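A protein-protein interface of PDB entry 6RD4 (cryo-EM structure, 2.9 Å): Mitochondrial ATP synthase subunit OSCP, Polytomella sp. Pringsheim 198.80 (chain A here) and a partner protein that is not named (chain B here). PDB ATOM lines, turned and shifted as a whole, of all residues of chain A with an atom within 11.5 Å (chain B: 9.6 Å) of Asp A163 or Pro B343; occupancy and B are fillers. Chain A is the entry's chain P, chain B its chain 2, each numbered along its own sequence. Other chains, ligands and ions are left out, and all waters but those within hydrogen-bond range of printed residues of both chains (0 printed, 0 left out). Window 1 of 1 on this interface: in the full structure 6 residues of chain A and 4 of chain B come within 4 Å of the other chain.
The guanidinium group (NH2) of Arg B342 is in salt-bridge range of the side-chain carboxylate (OE2) of Glu A160.
The backbone carbonyl oxygen (O) of Pro A161 sits at hydrogen-bond distance from the guanidinium group (NH1) of Arg B342 (3.0 Å).
The guanidinium group (NH1) of Arg B342 is in salt-bridge range of the side-chain carboxylate (OD1) of Asp A163, 3.5 Å away.
NH1 of Arg B342 lies within salt-bridge range of OE1 of Glu A166, 2.4 Å away.
The side-chain carboxylate (OE1) of Glu A166 lies within hydrogen-bond range of the backbone NH (N) of Asp A163, 3.4 Å away.
OG1 of Thr A158 is in hydrogen-bond range of O of Glu A160, at 3.3 Å.
N of Tyr B341 is in hydrogen-bond range of OE1 of Glu B344 (2.7 Å).
NH1 of Arg A167 sits at hydrogen-bond distance from O of Asp A163 (2.9 Å).
The backbone NH (N) of Gln B340 lies within hydrogen-bond range of the side-chain carboxylate (OE1) of Glu B344 (2.7 Å).
Asp A163 touches Tyr B341.
Asp A163 touches Pro B343 (OD2 to CD, 3.9 Å).
CD2 of Tyr B341 touches CD1 of Leu A165 (3.7 Å).
CB of Pro B343 touches CD2 of Leu A165, at 3.96 Å.
CD1 of Leu A165 touches OE2 of Glu B344 (3.3 Å).
CG of Glu A166 touches CD of Pro B343 (3.9 Å).
Glu A169 touches Pro B343.
Of the printed residues of chain B, Asp A163 touches Tyr B341, Arg B342 and Pro B343.
Leu A165 touches just these residues of chain B: Tyr B341, Pro B343 and Glu B344.
Tyr B341 touches just these residues of chain A: Asp A163 and Leu A165.
Of chain A, only Glu A160, Pro A161, Asp A163 and Glu A166 come within 4 Å of Arg B342.
Of the printed residues of chain A, Glu B344 touches Leu A165.
No residue of chain A comes within 4 Å of Ala B346.
No residue of chain A comes within 4 Å of Ser B347.
Printed residues of chain B within 4 Å of Pro A161: Arg B342 (3.0 Å).
Of the printed residues of chain B, Glu A160 touches Arg B342.
Of the printed residues of chain B, Glu A169 touches Pro B343 (3.3 Å).
Met A186 touches none of the printed residues of chain B.
The nearest printed residue of chain B that does not touch Glu A160 is Pro B343 (8.9 Å).
Of the 24 printed residues of chain A, 6 touch a printed residue of chain B.
Printed residues of chain A that touch a printed residue of chain B: Glu A160, Pro A161, Asp A163, Leu A165, Glu A166 and Glu A169.
Among the printed residues, Asp or Glu carboxylates within 4 Å of a Lys or Arg side-chain nitrogen of the other chain: Glu A160 with Arg B342 (3.4 Å), Asp A163 with Arg B342 (3.5 Å) and Glu A166 with Arg B342 (2.4 Å).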
ATOM      1  N   VAL A 156     -20.100 -21.693  33.091  1.00  0.00           N
ATOM      2  CA  VAL A 156     -19.585 -20.417  32.625  1.00  0.00           C
ATOM      3  C   VAL A 156     -20.763 -19.594  32.147  1.00  0.00           C
ATOM      4  O   VAL A 156     -21.535 -20.046  31.297  1.00  0.00           O
ATOM      5  CB  VAL A 156     -18.532 -20.577  31.525  1.00  0.00           C
ATOM      6  CG1 VAL A 156     -18.242 -19.248  30.908  1.00  0.00           C
ATOM      7  CG2 VAL A 156     -17.259 -21.125  32.115  1.00  0.00           C
ATOM      8  N   THR A 158     -21.633 -16.021  30.386  1.00  0.00           N
ATOM      9  CA  THR A 158     -21.069 -14.979  29.544  1.00  0.00           C
ATOM     10  C   THR A 158     -22.158 -13.979  29.168  1.00  0.00           C
ATOM     11  O   THR A 158     -23.283 -14.042  29.653  1.00  0.00           O
ATOM     12  CB  THR A 158     -20.422 -15.590  28.301  1.00  0.00           C
ATOM     13  OG1 THR A 158     -21.360 -16.463  27.665  1.00  0.00           O
ATOM     14  CG2 THR A 158     -19.187 -16.370  28.670  1.00  0.00           C
ATOM     15  N   ALA A 159     -21.807 -13.031  28.301  1.00  0.00           N
ATOM     16  CA  ALA A 159     -22.753 -11.979  27.950  1.00  0.00           C
ATOM     17  C   ALA A 159     -23.619 -12.383  26.760  1.00  0.00           C
ATOM     18  O   ALA A 159     -24.850 -12.284  26.809  1.00  0.00           O
ATOM     19  CB  ALA A 159     -22.000 -10.677  27.672  1.00  0.00           C
ATOM     20  N   GLU A 160     -22.991 -12.823  25.681  1.00  0.00           N
ATOM     21  CA  GLU A 160     -23.653 -13.397  24.522  1.00  0.00           C
ATOM     22  C   GLU A 160     -23.005 -14.747  24.255  1.00  0.00           C
ATOM     23  O   GLU A 160     -21.920 -15.019  24.779  1.00  0.00           O
ATOM     24  CB  GLU A 160     -23.533 -12.462  23.304  1.00  0.00           C
ATOM     25  CG  GLU A 160     -22.143 -12.327  22.728  1.00  0.00           C
ATOM     26  CD  GLU A 160     -21.370 -11.171  23.323  1.00  0.00           C
ATOM     27  OE1 GLU A 160     -21.786 -10.647  24.373  1.00  0.00           O
ATOM     28  OE2 GLU A 160     -20.345 -10.776  22.734  1.00  0.00           O
ATOM     29  N   PRO A 161     -23.667 -15.643  23.496  1.00  0.00           N
ATOM     30  CA  PRO A 161     -23.082 -16.965  23.232  1.00  0.00           C
ATOM     31  C   PRO A 161     -21.750 -16.907  22.500  1.00  0.00           C
ATOM     32  O   PRO A 161     -21.468 -15.984  21.737  1.00  0.00           O
ATOM     33  CB  PRO A 161     -24.146 -17.657  22.383  1.00  0.00           C
ATOM     34  CG  PRO A 161     -25.395 -17.091  22.861  1.00  0.00           C
ATOM     35  CD  PRO A 161     -25.104 -15.643  23.163  1.00  0.00           C
ATOM     36  N   LEU A 162     -20.928 -17.912  22.771  1.00  0.00           N
ATOM     37  CA  LEU A 162     -19.514 -17.873  22.469  1.00  0.00           C
ATOM     38  C   LEU A 162     -19.235 -18.231  21.015  1.00  0.00           C
ATOM     39  O   LEU A 162     -20.066 -18.800  20.306  1.00  0.00           O
ATOM     40  CB  LEU A 162     -18.751 -18.833  23.371  1.00  0.00           C
ATOM     41  CG  LEU A 162     -18.831 -18.635  24.876  1.00  0.00           C
ATOM     42  CD1 LEU A 162     -19.806 -19.618  25.475  1.00  0.00           C
ATOM     43  CD2 LEU A 162     -17.454 -18.826  25.451  1.00  0.00           C
ATOM     44  N   ASP A 163     -18.022 -17.898  20.589  1.00  0.00           N
ATOM     45  CA  ASP A 163     -17.446 -18.407  19.360  1.00  0.00           C
ATOM     46  C   ASP A 163     -16.892 -19.802  19.616  1.00  0.00           C
ATOM     47  O   ASP A 163     -16.992 -20.347  20.717  1.00  0.00           O
ATOM     48  CB  ASP A 163     -16.341 -17.479  18.868  1.00  0.00           C
ATOM     49  CG  ASP A 163     -16.774 -16.028  18.820  1.00  0.00           C
ATOM     50  OD1 ASP A 163     -17.992 -15.766  18.891  1.00  0.00           O
ATOM     51  OD2 ASP A 163     -15.897 -15.148  18.722  1.00  0.00           O
ATOM     52  N   LYS A 164     -16.285 -20.396  18.602  1.00  0.00           N
ATOM     53  CA  LYS A 164     -15.487 -21.573  18.880  1.00  0.00           C
ATOM     54  C   LYS A 164     -14.085 -21.194  19.330  1.00  0.00           C
ATOM     55  O   LYS A 164     -13.369 -22.047  19.853  1.00  0.00           O
ATOM     56  CB  LYS A 164     -15.446 -22.506  17.660  1.00  0.00           C
ATOM     57  CG  LYS A 164     -16.755 -23.182  17.259  1.00  0.00           C
ATOM     58  CD  LYS A 164     -16.585 -24.065  16.017  1.00  0.00           C
ATOM     59  CE  LYS A 164     -17.874 -24.745  15.642  1.00  0.00           C
ATOM     60  NZ  LYS A 164     -17.704 -25.576  14.427  1.00  0.00           N
ATOM     61  N   LEU A 165     -13.674 -19.944  19.113  1.00  0.00           N
ATOM     62  CA  LEU A 165     -12.400 -19.485  19.649  1.00  0.00           C
ATOM     63  C   LEU A 165     -12.594 -18.876  21.027  1.00  0.00           C
ATOM     64  O   LEU A 165     -11.700 -18.961  21.875  1.00  0.00           O
ATOM     65  CB  LEU A 165     -11.750 -18.480  18.699  1.00  0.00           C
ATOM     66  CG  LEU A 165     -10.222 -18.313  18.639  1.00  0.00           C
ATOM     67  CD1 LEU A 165      -9.885 -17.532  17.406  1.00  0.00           C
ATOM     68  CD2 LEU A 165      -9.582 -17.610  19.830  1.00  0.00           C
ATOM     69  N   GLU A 166     -13.764 -18.286  21.275  1.00  0.00           N
ATOM     70  CA  GLU A 166     -14.089 -17.831  22.623  1.00  0.00           C
ATOM     71  C   GLU A 166     -14.233 -19.001  23.586  1.00  0.00           C
ATOM     72  O   GLU A 166     -14.042 -18.836  24.793  1.00  0.00           O
ATOM     73  CB  GLU A 166     -15.369 -16.997  22.608  1.00  0.00           C
ATOM     74  CG  GLU A 166     -15.114 -15.502  22.540  1.00  0.00           C
ATOM     75  CD  GLU A 166     -16.361 -14.681  22.808  1.00  0.00           C
ATOM     76  OE1 GLU A 166     -17.476 -15.186  22.567  1.00  0.00           O
ATOM     77  OE2 GLU A 166     -16.224 -13.528  23.266  1.00  0.00           O
ATOM     78  N   ARG A 167     -14.572 -20.181  23.071  1.00  0.00           N
ATOM     79  CA  ARG A 167     -14.550 -21.386  23.885  1.00  0.00           C
ATOM     80  C   ARG A 167     -13.125 -21.814  24.208  1.00  0.00           C
ATOM     81  O   ARG A 167     -12.842 -22.237  25.331  1.00  0.00           O
ATOM     82  CB  ARG A 167     -15.290 -22.502  23.161  1.00  0.00           C
ATOM     83  CG  ARG A 167     -15.671 -23.673  24.020  1.00  0.00           C
ATOM     84  CD  ARG A 167     -16.793 -24.464  23.376  1.00  0.00           C
ATOM     85  NE  ARG A 167     -18.094 -23.830  23.566  1.00  0.00           N
ATOM     86  CZ  ARG A 167     -18.720 -23.106  22.646  1.00  0.00           C
ATOM     87  NH1 ARG A 167     -18.167 -22.909  21.463  1.00  0.00           N
ATOM     88  NH2 ARG A 167     -19.902 -22.571  22.913  1.00  0.00           N
ATOM     89  N   VAL A 168     -12.215 -21.716  23.242  1.00  0.00           N
ATOM     90  CA  VAL A 168     -10.890 -22.295  23.439  1.00  0.00           C
ATOM     91  C   VAL A 168     -10.005 -21.385  24.286  1.00  0.00           C
ATOM     92  O   VAL A 168      -9.202 -21.870  25.093  1.00  0.00           O
ATOM     93  CB  VAL A 168     -10.274 -22.619  22.064  1.00  0.00           C
ATOM     94  CG1 VAL A 168      -8.827 -23.060  22.169  1.00  0.00           C
ATOM     95  CG2 VAL A 168     -11.068 -23.725  21.405  1.00  0.00           C
ATOM     96  N   GLU A 169     -10.173 -20.067  24.171  1.00  0.00           N
ATOM     97  CA  GLU A 169      -9.387 -19.140  24.981  1.00  0.00           C
ATOM     98  C   GLU A 169      -9.830 -19.174  26.437  1.00  0.00           C
ATOM     99  O   GLU A 169      -9.078 -18.787  27.337  1.00  0.00           O
ATOM    100  CB  GLU A 169      -9.498 -17.721  24.424  1.00  0.00           C
ATOM    101  CG  GLU A 169     -10.906 -17.156  24.460  1.00  0.00           C
ATOM    102  CD  GLU A 169     -10.948 -15.644  24.554  1.00  0.00           C
ATOM    103  OE1 GLU A 169      -9.891 -15.021  24.784  1.00  0.00           O
ATOM    104  OE2 GLU A 169     -12.052 -15.080  24.401  1.00  0.00           O
ATOM    105  N   LEU A 170     -11.056 -19.631  26.681  1.00  0.00           N
ATOM    106  CA  LEU A 170     -11.642 -19.588  28.012  1.00  0.00           C
ATOM    107  C   LEU A 170     -11.198 -20.758  28.876  1.00  0.00           C
ATOM    108  O   LEU A 170     -11.009 -20.583  30.081  1.00  0.00           O
ATOM    109  CB  LEU A 170     -13.161 -19.564  27.883  1.00  0.00           C
ATOM    110  CG  LEU A 170     -14.117 -19.667  29.059  1.00  0.00           C
ATOM    111  CD1 LEU A 170     -13.739 -18.767  30.203  1.00  0.00           C
ATOM    112  CD2 LEU A 170     -15.457 -19.284  28.528  1.00  0.00           C
ATOM    113  N   THR A 171     -11.033 -21.947  28.295  1.00  0.00           N
ATOM    114  CA  THR A 171     -10.540 -23.075  29.075  1.00  0.00           C
ATOM    115  C   THR A 171      -9.097 -22.851  29.493  1.00  0.00           C
ATOM    116  O   THR A 171      -8.680 -23.276  30.573  1.00  0.00           O
ATOM    117  CB  THR A 171     -10.671 -24.377  28.290  1.00  0.00           C
ATOM    118  OG1 THR A 171      -9.650 -24.431  27.292  1.00  0.00           O
ATOM    119  CG2 THR A 171     -12.016 -24.453  27.629  1.00  0.00           C
ATOM    120  N   LYS A 172      -8.327 -22.161  28.654  1.00  0.00           N
ATOM    121  CA  LYS A 172      -6.983 -21.754  29.033  1.00  0.00           C
ATOM    122  C   LYS A 172      -6.981 -20.807  30.227  1.00  0.00           C
ATOM    123  O   LYS A 172      -6.007 -20.782  30.982  1.00  0.00           O
ATOM    124  CB  LYS A 172      -6.294 -21.097  27.839  1.00  0.00           C
ATOM    125  CG  LYS A 172      -6.227 -21.978  26.601  1.00  0.00           C
ATOM    126  CD  LYS A 172      -5.447 -23.262  26.849  1.00  0.00           C
ATOM    127  CE  LYS A 172      -3.992 -22.968  27.156  1.00  0.00           C
ATOM    128  NZ  LYS A 172      -3.329 -22.298  26.011  1.00  0.00           N
ATOM    129  N   LYS A 173      -8.053 -20.035  30.417  1.00  0.00           N
ATOM    130  CA  LYS A 173      -8.222 -19.286  31.655  1.00  0.00           C
ATOM    131  C   LYS A 173      -8.652 -20.204  32.790  1.00  0.00           C
ATOM    132  O   LYS A 173      -8.160 -20.085  33.917  1.00  0.00           O
ATOM    133  CB  LYS A 173      -9.268 -18.188  31.464  1.00  0.00           C
ATOM    134  CG  LYS A 173      -8.931 -17.133  30.445  1.00  0.00           C
ATOM    135  CD  LYS A 173      -7.897 -16.164  30.969  1.00  0.00           C
ATOM    136  CE  LYS A 173      -7.615 -15.086  29.946  1.00  0.00           C
ATOM    137  NZ  LYS A 173      -8.825 -14.254  29.713  1.00  0.00           N
ATOM    138  N   MET A 186     -17.858 -28.136  31.054  1.00  0.00           N
ATOM    139  CA  MET A 186     -18.192 -26.710  31.126  1.00  0.00           C
ATOM    140  C   MET A 186     -19.719 -26.720  31.137  1.00  0.00           C
ATOM    141  O   MET A 186     -20.319 -27.764  30.872  1.00  0.00           O
ATOM    142  CB  MET A 186     -17.616 -25.841  29.997  1.00  0.00           C
ATOM    143  CG  MET A 186     -17.613 -24.340  30.291  1.00  0.00           C
ATOM    144  SD  MET A 186     -16.787 -23.316  29.066  1.00  0.00           S
ATOM    145  CE  MET A 186     -15.084 -23.604  29.519  1.00  0.00           C
ATOM    146  N   GLU A 188     -22.551 -23.703  29.621  1.00  0.00           N
ATOM    147  CA  GLU A 188     -22.533 -22.358  29.062  1.00  0.00           C
ATOM    148  C   GLU A 188     -23.907 -21.717  29.200  1.00  0.00           C
ATOM    149  O   GLU A 188     -24.897 -22.234  28.675  1.00  0.00           O
ATOM    150  CB  GLU A 188     -22.079 -22.406  27.607  1.00  0.00           C
ATOM    151  CG  GLU A 188     -20.640 -22.867  27.481  1.00  0.00           C
ATOM    152  CD  GLU A 188     -20.208 -23.108  26.051  1.00  0.00           C
ATOM    153  OE1 GLU A 188     -21.071 -23.085  25.149  1.00  0.00           O
ATOM    154  OE2 GLU A 188     -18.997 -23.317  25.823  1.00  0.00           O
ATOM    155  N   LYS A 189     -23.957 -20.597  29.915  1.00  0.00           N
ATOM    156  CA  LYS A 189     -25.161 -19.804  30.096  1.00  0.00           C
ATOM    157  C   LYS A 189     -24.842 -18.360  29.744  1.00  0.00           C
ATOM    158  O   LYS A 189     -23.681 -17.986  29.581  1.00  0.00           O
ATOM    159  CB  LYS A 189     -25.696 -19.928  31.526  1.00  0.00           C
ATOM    160  CG  LYS A 189     -26.127 -21.343  31.879  1.00  0.00           C
ATOM    161  CD  LYS A 189     -27.318 -21.748  31.021  1.00  0.00           C
ATOM    162  CE  LYS A 189     -27.823 -23.139  31.344  1.00  0.00           C
ATOM    163  NZ  LYS A 189     -26.868 -24.180  30.874  1.00  0.00           N
ATOM    164  N   ILE A 190     -25.883 -17.545  29.577  1.00  0.00           N
ATOM    165  CA  ILE A 190     -25.701 -16.175  29.114  1.00  0.00           C
ATOM    166  C   ILE A 190     -26.392 -15.198  30.058  1.00  0.00           C
ATOM    167  O   ILE A 190     -27.429 -15.500  30.659  1.00  0.00           O
ATOM    168  CB  ILE A 190     -26.197 -15.968  27.663  1.00  0.00           C
ATOM    169  CG1 ILE A 190     -27.681 -16.289  27.526  1.00  0.00           C
ATOM    170  CG2 ILE A 190     -25.392 -16.795  26.686  1.00  0.00           C
ATOM    171  CD1 ILE A 190     -28.266 -15.856  26.199  1.00  0.00           C
ATOM    172  N   GLY A 196     -19.573  -8.485  29.134  1.00  0.00           N
ATOM    173  CA  GLY A 196     -18.410  -9.177  28.631  1.00  0.00           C
ATOM    174  C   GLY A 196     -17.518  -9.684  29.749  1.00  0.00           C
ATOM    175  O   GLY A 196     -17.635  -9.297  30.908  1.00  0.00           O
ATOM    176  N   GLY A 197     -16.591 -10.554  29.372  1.00  0.00           N
ATOM    177  CA  GLY A 197     -15.888 -11.344  30.357  1.00  0.00           C
ATOM    178  C   GLY A 197     -16.732 -12.562  30.655  1.00  0.00           C
ATOM    179  O   GLY A 197     -17.561 -12.949  29.826  1.00  0.00           O
ATOM    180  N   PHE A 198     -16.568 -13.156  31.830  1.00  0.00           N
ATOM    181  CA  PHE A 198     -17.321 -14.356  32.160  1.00  0.00           C
ATOM    182  C   PHE A 198     -17.384 -14.503  33.669  1.00  0.00           C
ATOM    183  O   PHE A 198     -16.660 -13.835  34.410  1.00  0.00           O
ATOM    184  CB  PHE A 198     -16.698 -15.606  31.539  1.00  0.00           C
ATOM    185  CG  PHE A 198     -15.207 -15.646  31.632  1.00  0.00           C
ATOM    186  CD1 PHE A 198     -14.424 -15.209  30.586  1.00  0.00           C
ATOM    187  CD2 PHE A 198     -14.585 -16.138  32.761  1.00  0.00           C
ATOM    188  CE1 PHE A 198     -13.057 -15.244  30.669  1.00  0.00           C
ATOM    189  CE2 PHE A 198     -13.219 -16.181  32.847  1.00  0.00           C
ATOM    190  CZ  PHE A 198     -12.455 -15.734  31.798  1.00  0.00           C
ATOM    191  N   ALA B 334     -10.722  -5.178  10.623  1.00  0.00           N
ATOM    192  CA  ALA B 334     -10.200  -6.449  11.108  1.00  0.00           C
ATOM    193  C   ALA B 334     -10.824  -7.622  10.360  1.00  0.00           C
ATOM    194  O   ALA B 334     -10.127  -8.574  10.003  1.00  0.00           O
ATOM    195  CB  ALA B 334     -10.437  -6.578  12.608  1.00  0.00           C
ATOM    196  N   GLY B 338      -9.151 -10.402   7.584  1.00  0.00           N
ATOM    197  CA  GLY B 338      -9.272 -11.797   7.939  1.00  0.00           C
ATOM    198  C   GLY B 338      -9.259 -11.983   9.433  1.00  0.00           C
ATOM    199  O   GLY B 338      -8.202 -12.155  10.045  1.00  0.00           O
ATOM    200  N   ALA B 339     -10.453 -11.968  10.016  1.00  0.00           N
ATOM    201  CA  ALA B 339     -10.651 -12.199  11.441  1.00  0.00           C
ATOM    202  C   ALA B 339     -12.130 -12.494  11.618  1.00  0.00           C
ATOM    203  O   ALA B 339     -12.946 -11.575  11.526  1.00  0.00           O
ATOM    204  CB  ALA B 339     -10.232 -10.990  12.262  1.00  0.00           C
ATOM    205  N   GLN B 340     -12.483 -13.747  11.868  1.00  0.00           N
ATOM    206  CA  GLN B 340     -13.893 -14.087  11.967  1.00  0.00           C
ATOM    207  C   GLN B 340     -14.379 -14.210  13.398  1.00  0.00           C
ATOM    208  O   GLN B 340     -15.590 -14.292  13.616  1.00  0.00           O
ATOM    209  CB  GLN B 340     -14.183 -15.391  11.214  1.00  0.00           C
ATOM    210  CG  GLN B 340     -13.592 -16.630  11.849  1.00  0.00           C
ATOM    211  CD  GLN B 340     -12.177 -16.913  11.391  1.00  0.00           C
ATOM    212  OE1 GLN B 340     -11.520 -16.066  10.790  1.00  0.00           O
ATOM    213  NE2 GLN B 340     -11.696 -18.111  11.687  1.00  0.00           N
ATOM    214  N   TYR B 341     -13.483 -14.196  14.374  1.00  0.00           N
ATOM    215  CA  TYR B 341     -13.864 -14.376  15.760  1.00  0.00           C
ATOM    216  C   TYR B 341     -13.483 -13.158  16.583  1.00  0.00           C
ATOM    217  O   TYR B 341     -12.587 -12.392  16.220  1.00  0.00           O
ATOM    218  CB  TYR B 341     -13.228 -15.636  16.339  1.00  0.00           C
ATOM    219  CG  TYR B 341     -13.698 -16.874  15.623  1.00  0.00           C
ATOM    220  CD1 TYR B 341     -15.041 -17.048  15.331  1.00  0.00           C
ATOM    221  CD2 TYR B 341     -12.803 -17.852  15.228  1.00  0.00           C
ATOM    222  CE1 TYR B 341     -15.483 -18.166  14.672  1.00  0.00           C
ATOM    223  CE2 TYR B 341     -13.233 -18.971  14.566  1.00  0.00           C
ATOM    224  CZ  TYR B 341     -14.575 -19.125  14.289  1.00  0.00           C
ATOM    225  OH  TYR B 341     -15.014 -20.248  13.626  1.00  0.00           O
ATOM    226  N   ARG B 342     -14.193 -12.990  17.695  1.00  0.00           N
ATOM    227  CA  ARG B 342     -14.034 -11.793  18.511  1.00  0.00           C
ATOM    228  C   ARG B 342     -12.686 -11.642  19.218  1.00  0.00           C
ATOM    229  O   ARG B 342     -12.252 -10.488  19.359  1.00  0.00           O
ATOM    230  CB  ARG B 342     -15.190 -11.716  19.514  1.00  0.00           C
ATOM    231  CG  ARG B 342     -16.534 -11.589  18.834  1.00  0.00           C
ATOM    232  CD  ARG B 342     -17.600 -11.189  19.818  1.00  0.00           C
ATOM    233  NE  ARG B 342     -17.926 -12.273  20.732  1.00  0.00           N
ATOM    234  CZ  ARG B 342     -19.085 -12.913  20.726  1.00  0.00           C
ATOM    235  NH1 ARG B 342     -19.310 -13.892  21.590  1.00  0.00           N
ATOM    236  NH2 ARG B 342     -20.021 -12.563  19.857  1.00  0.00           N
ATOM    237  N   PRO B 343     -11.983 -12.688  19.687  1.00  0.00           N
ATOM    238  CA  PRO B 343     -10.601 -12.459  20.143  1.00  0.00           C
ATOM    239  C   PRO B 343      -9.644 -12.059  19.038  1.00  0.00           C
ATOM    240  O   PRO B 343      -8.578 -11.511  19.337  1.00  0.00           O
ATOM    241  CB  PRO B 343     -10.201 -13.805  20.751  1.00  0.00           C
ATOM    242  CG  PRO B 343     -11.443 -14.362  21.211  1.00  0.00           C
ATOM    243  CD  PRO B 343     -12.455 -13.999  20.180  1.00  0.00           C
ATOM    244  N   GLU B 344      -9.973 -12.333  17.780  1.00  0.00           N
ATOM    245  CA  GLU B 344      -9.139 -11.854  16.690  1.00  0.00           C
ATOM    246  C   GLU B 344      -9.360 -10.369  16.436  1.00  0.00           C
ATOM    247  O   GLU B 344      -8.392  -9.609  16.315  1.00  0.00           O
ATOM    248  CB  GLU B 344      -9.425 -12.655  15.427  1.00  0.00           C
ATOM    249  CG  GLU B 344      -9.081 -14.118  15.494  1.00  0.00           C
ATOM    250  CD  GLU B 344      -9.949 -14.939  14.568  1.00  0.00           C
ATOM    251  OE1 GLU B 344     -10.857 -14.360  13.942  1.00  0.00           O
ATOM    252  OE2 GLU B 344      -9.707 -16.153  14.442  1.00  0.00           O
ATOM    253  N   VAL B 345     -10.625  -9.931  16.361  1.00  0.00           N
ATOM    254  CA  VAL B 345     -10.894  -8.532  16.052  1.00  0.00           C
ATOM    255  C   VAL B 345     -10.554  -7.646  17.241  1.00  0.00           C
ATOM    256  O   VAL B 345     -10.252  -6.466  17.075  1.00  0.00           O
ATOM    257  CB  VAL B 345     -12.351  -8.317  15.588  1.00  0.00           C
ATOM    258  CG1 VAL B 345     -12.666  -9.171  14.405  1.00  0.00           C
ATOM    259  CG2 VAL B 345     -13.343  -8.575  16.684  1.00  0.00           C
ATOM    260  N   ALA B 346     -10.575  -8.194  18.454  1.00  0.00           N
ATOM    261  CA  ALA B 346     -10.214  -7.376  19.601  1.00  0.00           C
ATOM    262  C   ALA B 346      -8.718  -7.131  19.659  1.00  0.00           C
ATOM    263  O   ALA B 346      -8.282  -6.077  20.130  1.00  0.00           O
ATOM    264  CB  ALA B 346     -10.690  -8.027  20.893  1.00  0.00           C
ATOM    265  N   SER B 347      -7.919  -8.076  19.185  1.00  0.00           N
ATOM    266  CA  SER B 347      -6.477  -7.913  19.186  1.00  0.00           C
ATOM    267  C   SER B 347      -5.948  -7.394  17.861  1.00  0.00           C
ATOM    268  O   SER B 347      -4.750  -7.116  17.758  1.00  0.00           O
ATOM    269  CB  SER B 347      -5.796  -9.237  19.535  1.00  0.00           C
ATOM    270  OG  SER B 347      -4.444  -9.237  19.119  1.00  0.00           O
ATOM    271  N   ALA B 348      -6.801  -7.266  16.846  1.00  0.00           N
ATOM    272  CA  ALA B 348      -6.374  -6.636  15.605  1.00  0.00           C
ATOM    273  C   ALA B 348      -6.507  -5.124  15.664  1.00  0.00           C
ATOM    274  O   ALA B 348      -5.586  -4.411  15.256  1.00  0.00           O
ATOM    275  CB  ALA B 348      -7.181  -7.176  14.423  1.00  0.00           C
ATOM    276  N   VAL B 349      -7.619  -4.621  16.212  1.00  0.00           N
ATOM    277  CA  VAL B 349      -7.837  -3.184  16.286  1.00  0.00           C
ATOM    278  C   VAL B 349      -6.988  -2.537  17.363  1.00  0.00           C
ATOM    279  O   VAL B 349      -6.924  -1.311  17.432  1.00  0.00           O
ATOM    280  CB  VAL B 349      -9.321  -2.857  16.514  1.00  0.00           C
ATOM    281  CG1 VAL B 349     -10.176  -3.614  15.561  1.00  0.00           C
ATOM    282  CG2 VAL B 349      -9.721  -3.150  17.924  1.00  0.00           C
ATOM    283  N   ALA B 350      -6.340  -3.312  18.212  1.00  0.00           N
ATOM    284  CA  ALA B 350      -5.311  -2.769  19.079  1.00  0.00           C
ATOM    285  C   ALA B 350      -3.953  -2.752  18.403  1.00  0.00           C
ATOM    286  O   ALA B 350      -2.986  -2.271  18.995  1.00  0.00           O
ATOM    287  CB  ALA B 350      -5.233  -3.568  20.378  1.00  0.00           C
ATOM    288  N   SER B 351      -3.853  -3.293  17.199  1.00  0.00           N
ATOM    289  CA  SER B 351      -2.639  -3.205  16.408  1.00  0.00           C
ATOM    290  C   SER B 351      -2.761  -2.199  15.281  1.00  0.00           C
ATOM    291  O   SER B 351      -1.768  -1.920  14.605  1.00  0.00           O
ATOM    292  CB  SER B 351      -2.289  -4.572  15.822  1.00  0.00           C
ATOM    293  OG  SER B 351      -3.369  -5.064  15.048  1.00  0.00           O
